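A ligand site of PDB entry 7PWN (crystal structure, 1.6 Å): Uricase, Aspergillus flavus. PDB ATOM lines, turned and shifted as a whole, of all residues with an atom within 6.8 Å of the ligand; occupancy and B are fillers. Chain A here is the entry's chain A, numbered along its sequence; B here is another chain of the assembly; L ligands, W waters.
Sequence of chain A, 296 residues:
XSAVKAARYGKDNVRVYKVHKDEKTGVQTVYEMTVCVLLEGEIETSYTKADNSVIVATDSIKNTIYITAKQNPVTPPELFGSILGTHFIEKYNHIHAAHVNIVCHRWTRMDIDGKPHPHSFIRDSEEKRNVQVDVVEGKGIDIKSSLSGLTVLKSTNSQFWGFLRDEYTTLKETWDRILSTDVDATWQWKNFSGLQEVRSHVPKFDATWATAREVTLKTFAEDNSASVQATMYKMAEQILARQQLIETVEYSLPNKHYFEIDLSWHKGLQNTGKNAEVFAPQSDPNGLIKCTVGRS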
ATOM      1  N   SER A 158      31.628  19.826  -1.387  1.00  0.00           N
ATOM      2  CA  SER A 158      31.017  19.249  -0.177  1.00  0.00           C
ATOM      3  C   SER A 158      31.919  18.115   0.274  1.00  0.00           C
ATOM      4  O   SER A 158      32.391  17.346  -0.578  1.00  0.00           O
ATOM      5  CB  SER A 158      29.598  18.794  -0.472  1.00  0.00           C
ATOM      6  OG  SER A 158      29.041  18.143   0.648  1.00  0.00           O
ATOM      7  N   GLN A 159      32.119  18.018   1.588  1.00  0.00           N
ATOM      8  CA  GLN A 159      32.986  17.019   2.242  1.00  0.00           C
ATOM      9  C   GLN A 159      32.261  16.470   3.451  1.00  0.00           C
ATOM     10  O   GLN A 159      31.421  17.178   4.024  1.00  0.00           O
ATOM     11  CB  GLN A 159      34.297  17.689   2.668  1.00  0.00           C
ATOM     12  CG  GLN A 159      34.985  18.425   1.533  1.00  0.00           C
ATOM     13  CD  GLN A 159      36.358  18.885   1.977  1.00  0.00           C
ATOM     14  OE1 GLN A 159      37.044  18.201   2.725  1.00  0.00           O
ATOM     15  NE2 GLN A 159      36.742  20.062   1.531  1.00  0.00           N
ATOM     16  N   PHE A 160      32.621  15.281   3.872  1.00  0.00           N
ATOM     17  CA  PHE A 160      32.141  14.729   5.157  1.00  0.00           C
ATOM     18  C   PHE A 160      33.138  13.686   5.651  1.00  0.00           C
ATOM     19  O   PHE A 160      33.129  12.524   5.200  1.00  0.00           O
ATOM     20  CB  PHE A 160      30.715  14.197   5.057  1.00  0.00           C
ATOM     21  CG  PHE A 160      30.114  13.959   6.414  1.00  0.00           C
ATOM     22  CD1 PHE A 160      29.993  15.019   7.301  1.00  0.00           C
ATOM     23  CD2 PHE A 160      29.804  12.691   6.839  1.00  0.00           C
ATOM     24  CE1 PHE A 160      29.469  14.811   8.566  1.00  0.00           C
ATOM     25  CE2 PHE A 160      29.281  12.486   8.112  1.00  0.00           C
ATOM     26  CZ  PHE A 160      29.140  13.550   8.980  1.00  0.00           C
ATOM     27  N   PHE A 163      33.991  12.153  11.280  1.00  0.00           N
ATOM     28  CA  PHE A 163      32.856  11.817  12.163  1.00  0.00           C
ATOM     29  C   PHE A 163      33.235  10.621  13.021  1.00  0.00           C
ATOM     30  O   PHE A 163      34.221   9.927  12.699  1.00  0.00           O
ATOM     31  CB  PHE A 163      31.591  11.525  11.347  1.00  0.00           C
ATOM     32  CG  PHE A 163      31.838  10.698  10.112  1.00  0.00           C
ATOM     33  CD1 PHE A 163      32.183  11.293   8.901  1.00  0.00           C
ATOM     34  CD2 PHE A 163      31.702   9.320  10.166  1.00  0.00           C
ATOM     35  CE1 PHE A 163      32.397  10.520   7.772  1.00  0.00           C
ATOM     36  CE2 PHE A 163      31.911   8.557   9.022  1.00  0.00           C
ATOM     37  CZ  PHE A 163      32.256   9.155   7.843  1.00  0.00           C
ATOM     38  N   LEU A 171      30.069   4.126   6.880  1.00  0.00           N
ATOM     39  CA  LEU A 171      30.237   5.263   5.944  1.00  0.00           C
ATOM     40  C   LEU A 171      31.725   5.562   5.742  1.00  0.00           C
ATOM     41  O   LEU A 171      32.451   5.828   6.735  1.00  0.00           O
ATOM     42  CB  LEU A 171      29.494   6.470   6.495  1.00  0.00           C
ATOM     43  CG  LEU A 171      29.550   7.737   5.626  1.00  0.00           C
ATOM     44  CD1 LEU A 171      28.920   7.511   4.260  1.00  0.00           C
ATOM     45  CD2 LEU A 171      28.863   8.902   6.326  1.00  0.00           C
ATOM     46  N   ARG A 177      31.984  15.203  -2.441  1.00  0.00           N
ATOM     47  CA  ARG A 177      30.678  14.549  -2.656  1.00  0.00           C
ATOM     48  C   ARG A 177      29.688  15.559  -3.204  1.00  0.00           C
ATOM     49  O   ARG A 177      29.990  16.788  -3.262  1.00  0.00           O
ATOM     50  CB  ARG A 177      30.127  13.947  -1.360  1.00  0.00           C
ATOM     51  CG  ARG A 177      29.804  14.981  -0.293  1.00  0.00           C
ATOM     52  CD  ARG A 177      29.222  14.401   0.978  1.00  0.00           C
ATOM     53  NE  ARG A 177      28.744  15.482   1.826  1.00  0.00           N
ATOM     54  CZ  ARG A 177      28.047  15.323   2.950  1.00  0.00           C
ATOM     55  NH1 ARG A 177      27.814  14.123   3.432  1.00  0.00           N
ATOM     56  NH2 ARG A 177      27.667  16.402   3.627  1.00  0.00           N
ATOM     57  N   LEU A 179      26.111  17.486  -2.729  1.00  0.00           N
ATOM     58  CA  LEU A 179      25.193  17.888  -1.658  1.00  0.00           C
ATOM     59  C   LEU A 179      23.940  18.480  -2.284  1.00  0.00           C
ATOM     60  O   LEU A 179      24.032  19.392  -3.116  1.00  0.00           O
ATOM     61  CB  LEU A 179      25.891  18.910  -0.744  1.00  0.00           C
ATOM     62  CG  LEU A 179      25.029  19.509   0.369  1.00  0.00           C
ATOM     63  CD1 LEU A 179      24.494  18.435   1.283  1.00  0.00           C
ATOM     64  CD2 LEU A 179      25.852  20.524   1.164  1.00  0.00           C
ATOM     65  N   SER A 225      31.867  22.906   1.948  1.00  0.00           N
ATOM     66  CA  SER A 225      31.066  22.490   3.106  1.00  0.00           C
ATOM     67  C   SER A 225      31.772  21.372   3.872  1.00  0.00           C
ATOM     68  O   SER A 225      32.013  20.294   3.286  1.00  0.00           O
ATOM     69  CB  SER A 225      29.670  22.051   2.669  1.00  0.00           C
ATOM     70  OG  SER A 225      28.961  21.513   3.772  1.00  0.00           O
ATOM     71  N   ALA A 226      31.932  21.539   5.175  1.00  0.00           N
ATOM     72  CA  ALA A 226      32.465  20.505   6.091  1.00  0.00           C
ATOM     73  C   ALA A 226      31.369  19.481   6.445  1.00  0.00           C
ATOM     74  O   ALA A 226      31.714  18.405   6.955  1.00  0.00           O
ATOM     75  CB  ALA A 226      33.022  21.164   7.341  1.00  0.00           C
ATOM     76  N   SER A 227      30.107  19.911   6.355  1.00  0.00           N
ATOM     77  CA  SER A 227      28.890  19.183   6.799  1.00  0.00           C
ATOM     78  C   SER A 227      27.692  20.058   6.497  1.00  0.00           C
ATOM     79  O   SER A 227      27.859  21.271   6.328  1.00  0.00           O
ATOM     80  CB  SER A 227      28.902  18.809   8.270  1.00  0.00           C
ATOM     81  OG  SER A 227      28.781  19.936   9.109  1.00  0.00           O
ATOM     82  N   VAL A 228      26.513  19.450   6.437  1.00  0.00           N
ATOM     83  CA  VAL A 228      25.262  20.242   6.386  1.00  0.00           C
ATOM     84  C   VAL A 228      25.256  21.189   7.593  1.00  0.00           C
ATOM     85  O   VAL A 228      24.906  22.371   7.424  1.00  0.00           O
ATOM     86  CB  VAL A 228      24.045  19.312   6.352  1.00  0.00           C
ATOM     87  CG1 VAL A 228      22.753  20.100   6.464  1.00  0.00           C
ATOM     88  CG2 VAL A 228      24.081  18.473   5.085  1.00  0.00           C
ATOM     89  N   GLN A 229      25.569  20.652   8.766  1.00  0.00           N
ATOM     90  CA  GLN A 229      25.598  21.359  10.074  1.00  0.00           C
ATOM     91  C   GLN A 229      26.382  22.665   9.928  1.00  0.00           C
ATOM     92  O   GLN A 229      25.863  23.733  10.297  1.00  0.00           O
ATOM     93  CB  GLN A 229      26.196  20.423  11.136  1.00  0.00           C
ATOM     94  CG  GLN A 229      25.294  19.285  11.587  1.00  0.00           C
ATOM     95  CD  GLN A 229      25.436  18.000  10.807  1.00  0.00           C
ATOM     96  OE1 GLN A 229      25.734  17.989   9.608  1.00  0.00           O
ATOM     97  NE2 GLN A 229      25.200  16.892  11.482  1.00  0.00           N
ATOM     98  N   ASN A 255      19.407  15.770   3.895  1.00  0.00           N
ATOM     99  CA  ASN A 255      20.583  15.406   3.089  1.00  0.00           C
ATOM    100  C   ASN A 255      20.108  14.376   2.060  1.00  0.00           C
ATOM    101  O   ASN A 255      19.849  13.253   2.450  1.00  0.00           O
ATOM    102  CB  ASN A 255      21.700  14.877   3.978  1.00  0.00           C
ATOM    103  CG  ASN A 255      23.053  14.882   3.296  1.00  0.00           C
ATOM    104  OD1 ASN A 255      23.179  15.301   2.142  1.00  0.00           O
ATOM    105  ND2 ASN A 255      24.056  14.413   4.018  1.00  0.00           N
ATOM    106  N   HIS A 257      20.686  12.139  -0.486  1.00  0.00           N
ATOM    107  CA  HIS A 257      21.934  11.405  -0.808  1.00  0.00           C
ATOM    108  C   HIS A 257      21.967  11.055  -2.292  1.00  0.00           C
ATOM    109  O   HIS A 257      20.961  10.555  -2.822  1.00  0.00           O
ATOM    110  CB  HIS A 257      22.070  10.175   0.087  1.00  0.00           C
ATOM    111  CG  HIS A 257      21.933  10.476   1.545  1.00  0.00           C
ATOM    112  ND1 HIS A 257      22.860  11.236   2.225  1.00  0.00           N
ATOM    113  CD2 HIS A 257      21.007  10.092   2.441  1.00  0.00           C
ATOM    114  CE1 HIS A 257      22.496  11.319   3.496  1.00  0.00           C
ATOM    115  NE2 HIS A 257      21.353  10.630   3.659  1.00  0.00           N
ATOM    116  N   GLY A 287      19.328  11.824   5.549  1.00  0.00           N
ATOM    117  CA  GLY A 287      19.773  12.725   6.624  1.00  0.00           C
ATOM    118  C   GLY A 287      18.724  13.799   6.870  1.00  0.00           C
ATOM    119  O   GLY A 287      18.158  14.346   5.904  1.00  0.00           O
ATOM    120  N   ILE A 289      18.802  17.344   9.228  1.00  0.00           N
ATOM    121  CA  ILE A 289      19.700  18.172  10.073  1.00  0.00           C
ATOM    122  C   ILE A 289      18.961  19.451  10.441  1.00  0.00           C
ATOM    123  O   ILE A 289      18.477  20.145   9.532  1.00  0.00           O
ATOM    124  CB  ILE A 289      21.044  18.427   9.369  1.00  0.00           C
ATOM    125  CG1 ILE A 289      21.738  17.117   9.010  1.00  0.00           C
ATOM    126  CG2 ILE A 289      21.941  19.325  10.219  1.00  0.00           C
ATOM    127  CD1 ILE A 289      21.391  16.594   7.644  1.00  0.00           C
ATOM    128  N   TYR B   9      19.622  16.194  14.874  1.00  0.00           N
ATOM    129  CA  TYR B   9      20.010  15.672  13.545  1.00  0.00           C
ATOM    130  C   TYR B   9      19.937  14.155  13.599  1.00  0.00           C
ATOM    131  O   TYR B   9      19.964  13.524  14.689  1.00  0.00           O
ATOM    132  CB  TYR B   9      21.403  16.186  13.165  1.00  0.00           C
ATOM    133  CG  TYR B   9      22.476  15.282  13.721  1.00  0.00           C
ATOM    134  CD1 TYR B   9      22.717  15.235  15.084  1.00  0.00           C
ATOM    135  CD2 TYR B   9      23.021  14.272  12.942  1.00  0.00           C
ATOM    136  CE1 TYR B   9      23.594  14.307  15.631  1.00  0.00           C
ATOM    137  CE2 TYR B   9      23.902  13.348  13.454  1.00  0.00           C
ATOM    138  CZ  TYR B   9      24.184  13.360  14.807  1.00  0.00           C
ATOM    139  OH  TYR B   9      25.056  12.438  15.309  1.00  0.00           O
ATOM    140  N   GLY B  10      19.746  13.548  12.434  1.00  0.00           N
ATOM    141  CA  GLY B  10      19.734  12.085  12.346  1.00  0.00           C
ATOM    142  C   GLY B  10      19.161  11.629  11.028  1.00  0.00           C
ATOM    143  O   GLY B  10      19.477  12.274   9.999  1.00  0.00           O
ATOM    144  N   LYS B  11      18.526  10.470  11.021  1.00  0.00           N
ATOM    145  CA  LYS B  11      18.078   9.847   9.759  1.00  0.00           C
ATOM    146  C   LYS B  11      16.562   9.718   9.788  1.00  0.00           C
ATOM    147  O   LYS B  11      16.017   9.212  10.771  1.00  0.00           O
ATOM    148  CB  LYS B  11      18.732   8.502   9.454  1.00  0.00           C
ATOM    149  CG  LYS B  11      18.548   8.085   8.005  1.00  0.00           C
ATOM    150  CD  LYS B  11      19.435   8.821   7.084  1.00  0.00           C
ATOM    151  CE  LYS B  11      20.746   8.120   6.858  1.00  0.00           C
ATOM    152  NZ  LYS B  11      21.742   9.017   6.235  1.00  0.00           N
ATOM    153  N   ASN B  52      33.389  17.537  13.322  1.00  0.00           N
ATOM    154  CA  ASN B  52      32.578  16.345  12.968  1.00  0.00           C
ATOM    155  C   ASN B  52      32.887  15.224  13.972  1.00  0.00           C
ATOM    156  O   ASN B  52      32.083  14.275  14.055  1.00  0.00           O
ATOM    157  CB  ASN B  52      32.816  15.909  11.523  1.00  0.00           C
ATOM    158  CG  ASN B  52      32.189  16.845  10.521  1.00  0.00           C
ATOM    159  OD1 ASN B  52      31.341  17.672  10.851  1.00  0.00           O
ATOM    160  ND2 ASN B  52      32.606  16.735   9.273  1.00  0.00           N
ATOM    161  N   ILE B  55      29.878  14.005  15.681  1.00  0.00           N
ATOM    162  CA  ILE B  55      28.733  13.463  14.888  1.00  0.00           C
ATOM    163  C   ILE B  55      28.793  11.937  14.877  1.00  0.00           C
ATOM    164  O   ILE B  55      29.765  11.391  14.312  1.00  0.00           O
ATOM    165  CB  ILE B  55      28.692  14.053  13.478  1.00  0.00           C
ATOM    166  CG1 ILE B  55      28.566  15.573  13.514  1.00  0.00           C
ATOM    167  CG2 ILE B  55      27.552  13.411  12.680  1.00  0.00           C
ATOM    168  CD1 ILE B  55      28.823  16.218  12.179  1.00  0.00           C
ATOM    169  N   VAL B  56      27.742  11.303  15.393  1.00  0.00           N
ATOM    170  CA  VAL B  56      27.337   9.909  15.055  1.00  0.00           C
ATOM    171  C   VAL B  56      26.637   9.993  13.698  1.00  0.00           C
ATOM    172  O   VAL B  56      25.549  10.596  13.638  1.00  0.00           O
ATOM    173  CB  VAL B  56      26.422   9.312  16.123  1.00  0.00           C
ATOM    174  CG1 VAL B  56      25.953   7.908  15.757  1.00  0.00           C
ATOM    175  CG2 VAL B  56      27.095   9.331  17.487  1.00  0.00           C
ATOM    176  N   ALA B  57      27.318   9.562  12.628  1.00  0.00           N
ATOM    177  CA  ALA B  57      26.881   9.763  11.240  1.00  0.00           C
ATOM    178  C   ALA B  57      25.421   9.317  11.080  1.00  0.00           C
ATOM    179  O   ALA B  57      25.013   8.306  11.704  1.00  0.00           O
ATOM    180  CB  ALA B  57      27.803   9.023  10.293  1.00  0.00           C
ATOM    181  N   THR B  58      24.609  10.084  10.344  1.00  0.00           N
ATOM    182  CA  THR B  58      23.205   9.672  10.072  1.00  0.00           C
ATOM    183  C   THR B  58      23.223   8.277   9.448  1.00  0.00           C
ATOM    184  O   THR B  58      22.309   7.492   9.715  1.00  0.00           O
ATOM    185  CB  THR B  58      22.468  10.715   9.223  1.00  0.00           C
ATOM    186  OG1 THR B  58      22.979  10.752   7.899  1.00  0.00           O
ATOM    187  CG2 THR B  58      22.521  12.090   9.854  1.00  0.00           C
ATOM    188  N   ASP B  59      24.211   7.987   8.603  1.00  0.00           N
ATOM    189  CA  ASP B  59      24.364   6.651   7.995  1.00  0.00           C
ATOM    190  C   ASP B  59      24.505   5.598   9.102  1.00  0.00           C
ATOM    191  O   ASP B  59      23.901   4.511   8.995  1.00  0.00           O
ATOM    192  CB  ASP B  59      25.543   6.612   7.024  1.00  0.00           C
ATOM    193  CG  ASP B  59      25.579   5.329   6.231  1.00  0.00           C
ATOM    194  OD1 ASP B  59      24.843   5.260   5.216  1.00  0.00           O
ATOM    195  OD2 ASP B  59      26.296   4.389   6.693  1.00  0.00           O
ATOM    196  N   SER B  60      25.240   5.907  10.164  1.00  0.00           N
ATOM    197  CA  SER B  60      25.441   4.984  11.317  1.00  0.00           C
ATOM    198  C   SER B  60      24.139   4.836  12.101  1.00  0.00           C
ATOM    199  O   SER B  60      23.815   3.727  12.530  1.00  0.00           O
ATOM    200  CB  SER B  60      26.580   5.475  12.208  1.00  0.00           C
ATOM    201  OG  SER B  60      27.768   5.617  11.437  1.00  0.00           O
HETATM  202  N1  LIG L   1      26.009  15.496   8.184  1.00  0.00           N
HETATM  203  C1  LIG L   1      26.410  15.515   6.876  1.00  0.00           C
HETATM  204  O1  LIG L   1      26.586  16.565   6.290  1.00  0.00           O
HETATM  205  N2  LIG L   1      26.479  14.331   6.190  1.00  0.00           N
HETATM  206  C2  LIG L   1      26.337  13.179   6.832  1.00  0.00           C
HETATM  207  C3  LIG L   1      26.021  13.145   8.174  1.00  0.00           C
HETATM  208  C4  LIG L   1      25.833  14.339   8.921  1.00  0.00           C
HETATM  209  O2  LIG L   1      25.500  14.423  10.109  1.00  0.00           O
HETATM  210  N3  LIG L   1      25.894  11.838   8.547  1.00  0.00           N
HETATM  211  N4  LIG L   1      26.130  11.089   7.491  1.00  0.00           N
HETATM  212  N5  LIG L   1      26.391  11.885   6.445  1.00  0.00           N
HETATM  213  O   HOH W   1      26.634  10.980   3.755  1.00  0.00           O
HETATM  214  O   HOH W   2      22.984  13.237   6.627  1.00  0.00           O
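The backbone NH of Val 228 lies within hydrogen-bond range of an oxygen (O1) of the ligand (2.9 Å). N3 of the ligand sits at hydrogen-bond distance from OG1 of Thr 58 of chain B (3.2 Å). NH2 of Arg 177 lies within hydrogen-bond range of O1 of the ligand, 2.9 Å away. An oxygen (O2) of the ligand lies within hydrogen-bond range of the side-chain amide nitrogen (NE2) of Gln 229, 2.8 Å away. The side-chain amide nitrogen (ND2) of Asn 255 lies close to a nitrogen (N2) of the ligand, at 3.3 Å. N3 of the ligand is in hydrogen-bond range of N of Thr 58 of chain B, at 2.8 Å.
The side-chain hydroxyl (OG1) of Thr 58 of chain B sits at hydrogen-bond distance from the side-chain amino group (NZ) of Lys 11 of chain B, at 2.7 Å. The backbone carbonyl oxygen (O) of Asn 255 lies within hydrogen-bond range of a ring nitrogen (NE2) of His 257 (3.3 Å). N of Arg 177 lies within hydrogen-bond range of O of Ser 158 (2.9 Å). The side-chain hydroxyl (OG) of Ser 227 sits close to the backbone NH (N) of Gln 229, 3.3 Å away. The side-chain hydroxyl of Ser 225 sits at hydrogen-bond distance from the backbone carbonyl oxygen of Ser 227, at 2.8 Å. The side-chain hydroxyl (OH) of Tyr 9 of chain B lies within hydrogen-bond range of the backbone carbonyl oxygen (O) of Val 56 of chain B, at 2.5 Å. The backbone carbonyl oxygen (O) of Gly 287 lies within hydrogen-bond range of the backbone NH (N) of Asn 255 (2.8 Å).
Residues that only touch the ligand: Phe 160, Ile 55 of chain B, Ser 227, Ala 57 of chain B, Leu 171, Tyr 9 of chain B and Asp 59 of chain B. Hydrophobic or aromatic side chains that line the ligand: Phe 160, Leu 171, Val 228, Tyr 9 of chain B, Ile 55 of chain B and Ala 57 of chain B.
Water W1 bridges a nitrogen (N5) of the ligand (2.8 Å) and the guanidinium group of Arg 177 (3.4 Å). Water W2 lies within hydrogen-bond range of OG1 of Thr 58 of chain B (2.8 Å) and ND2 of Asn 255 (3.1 Å).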
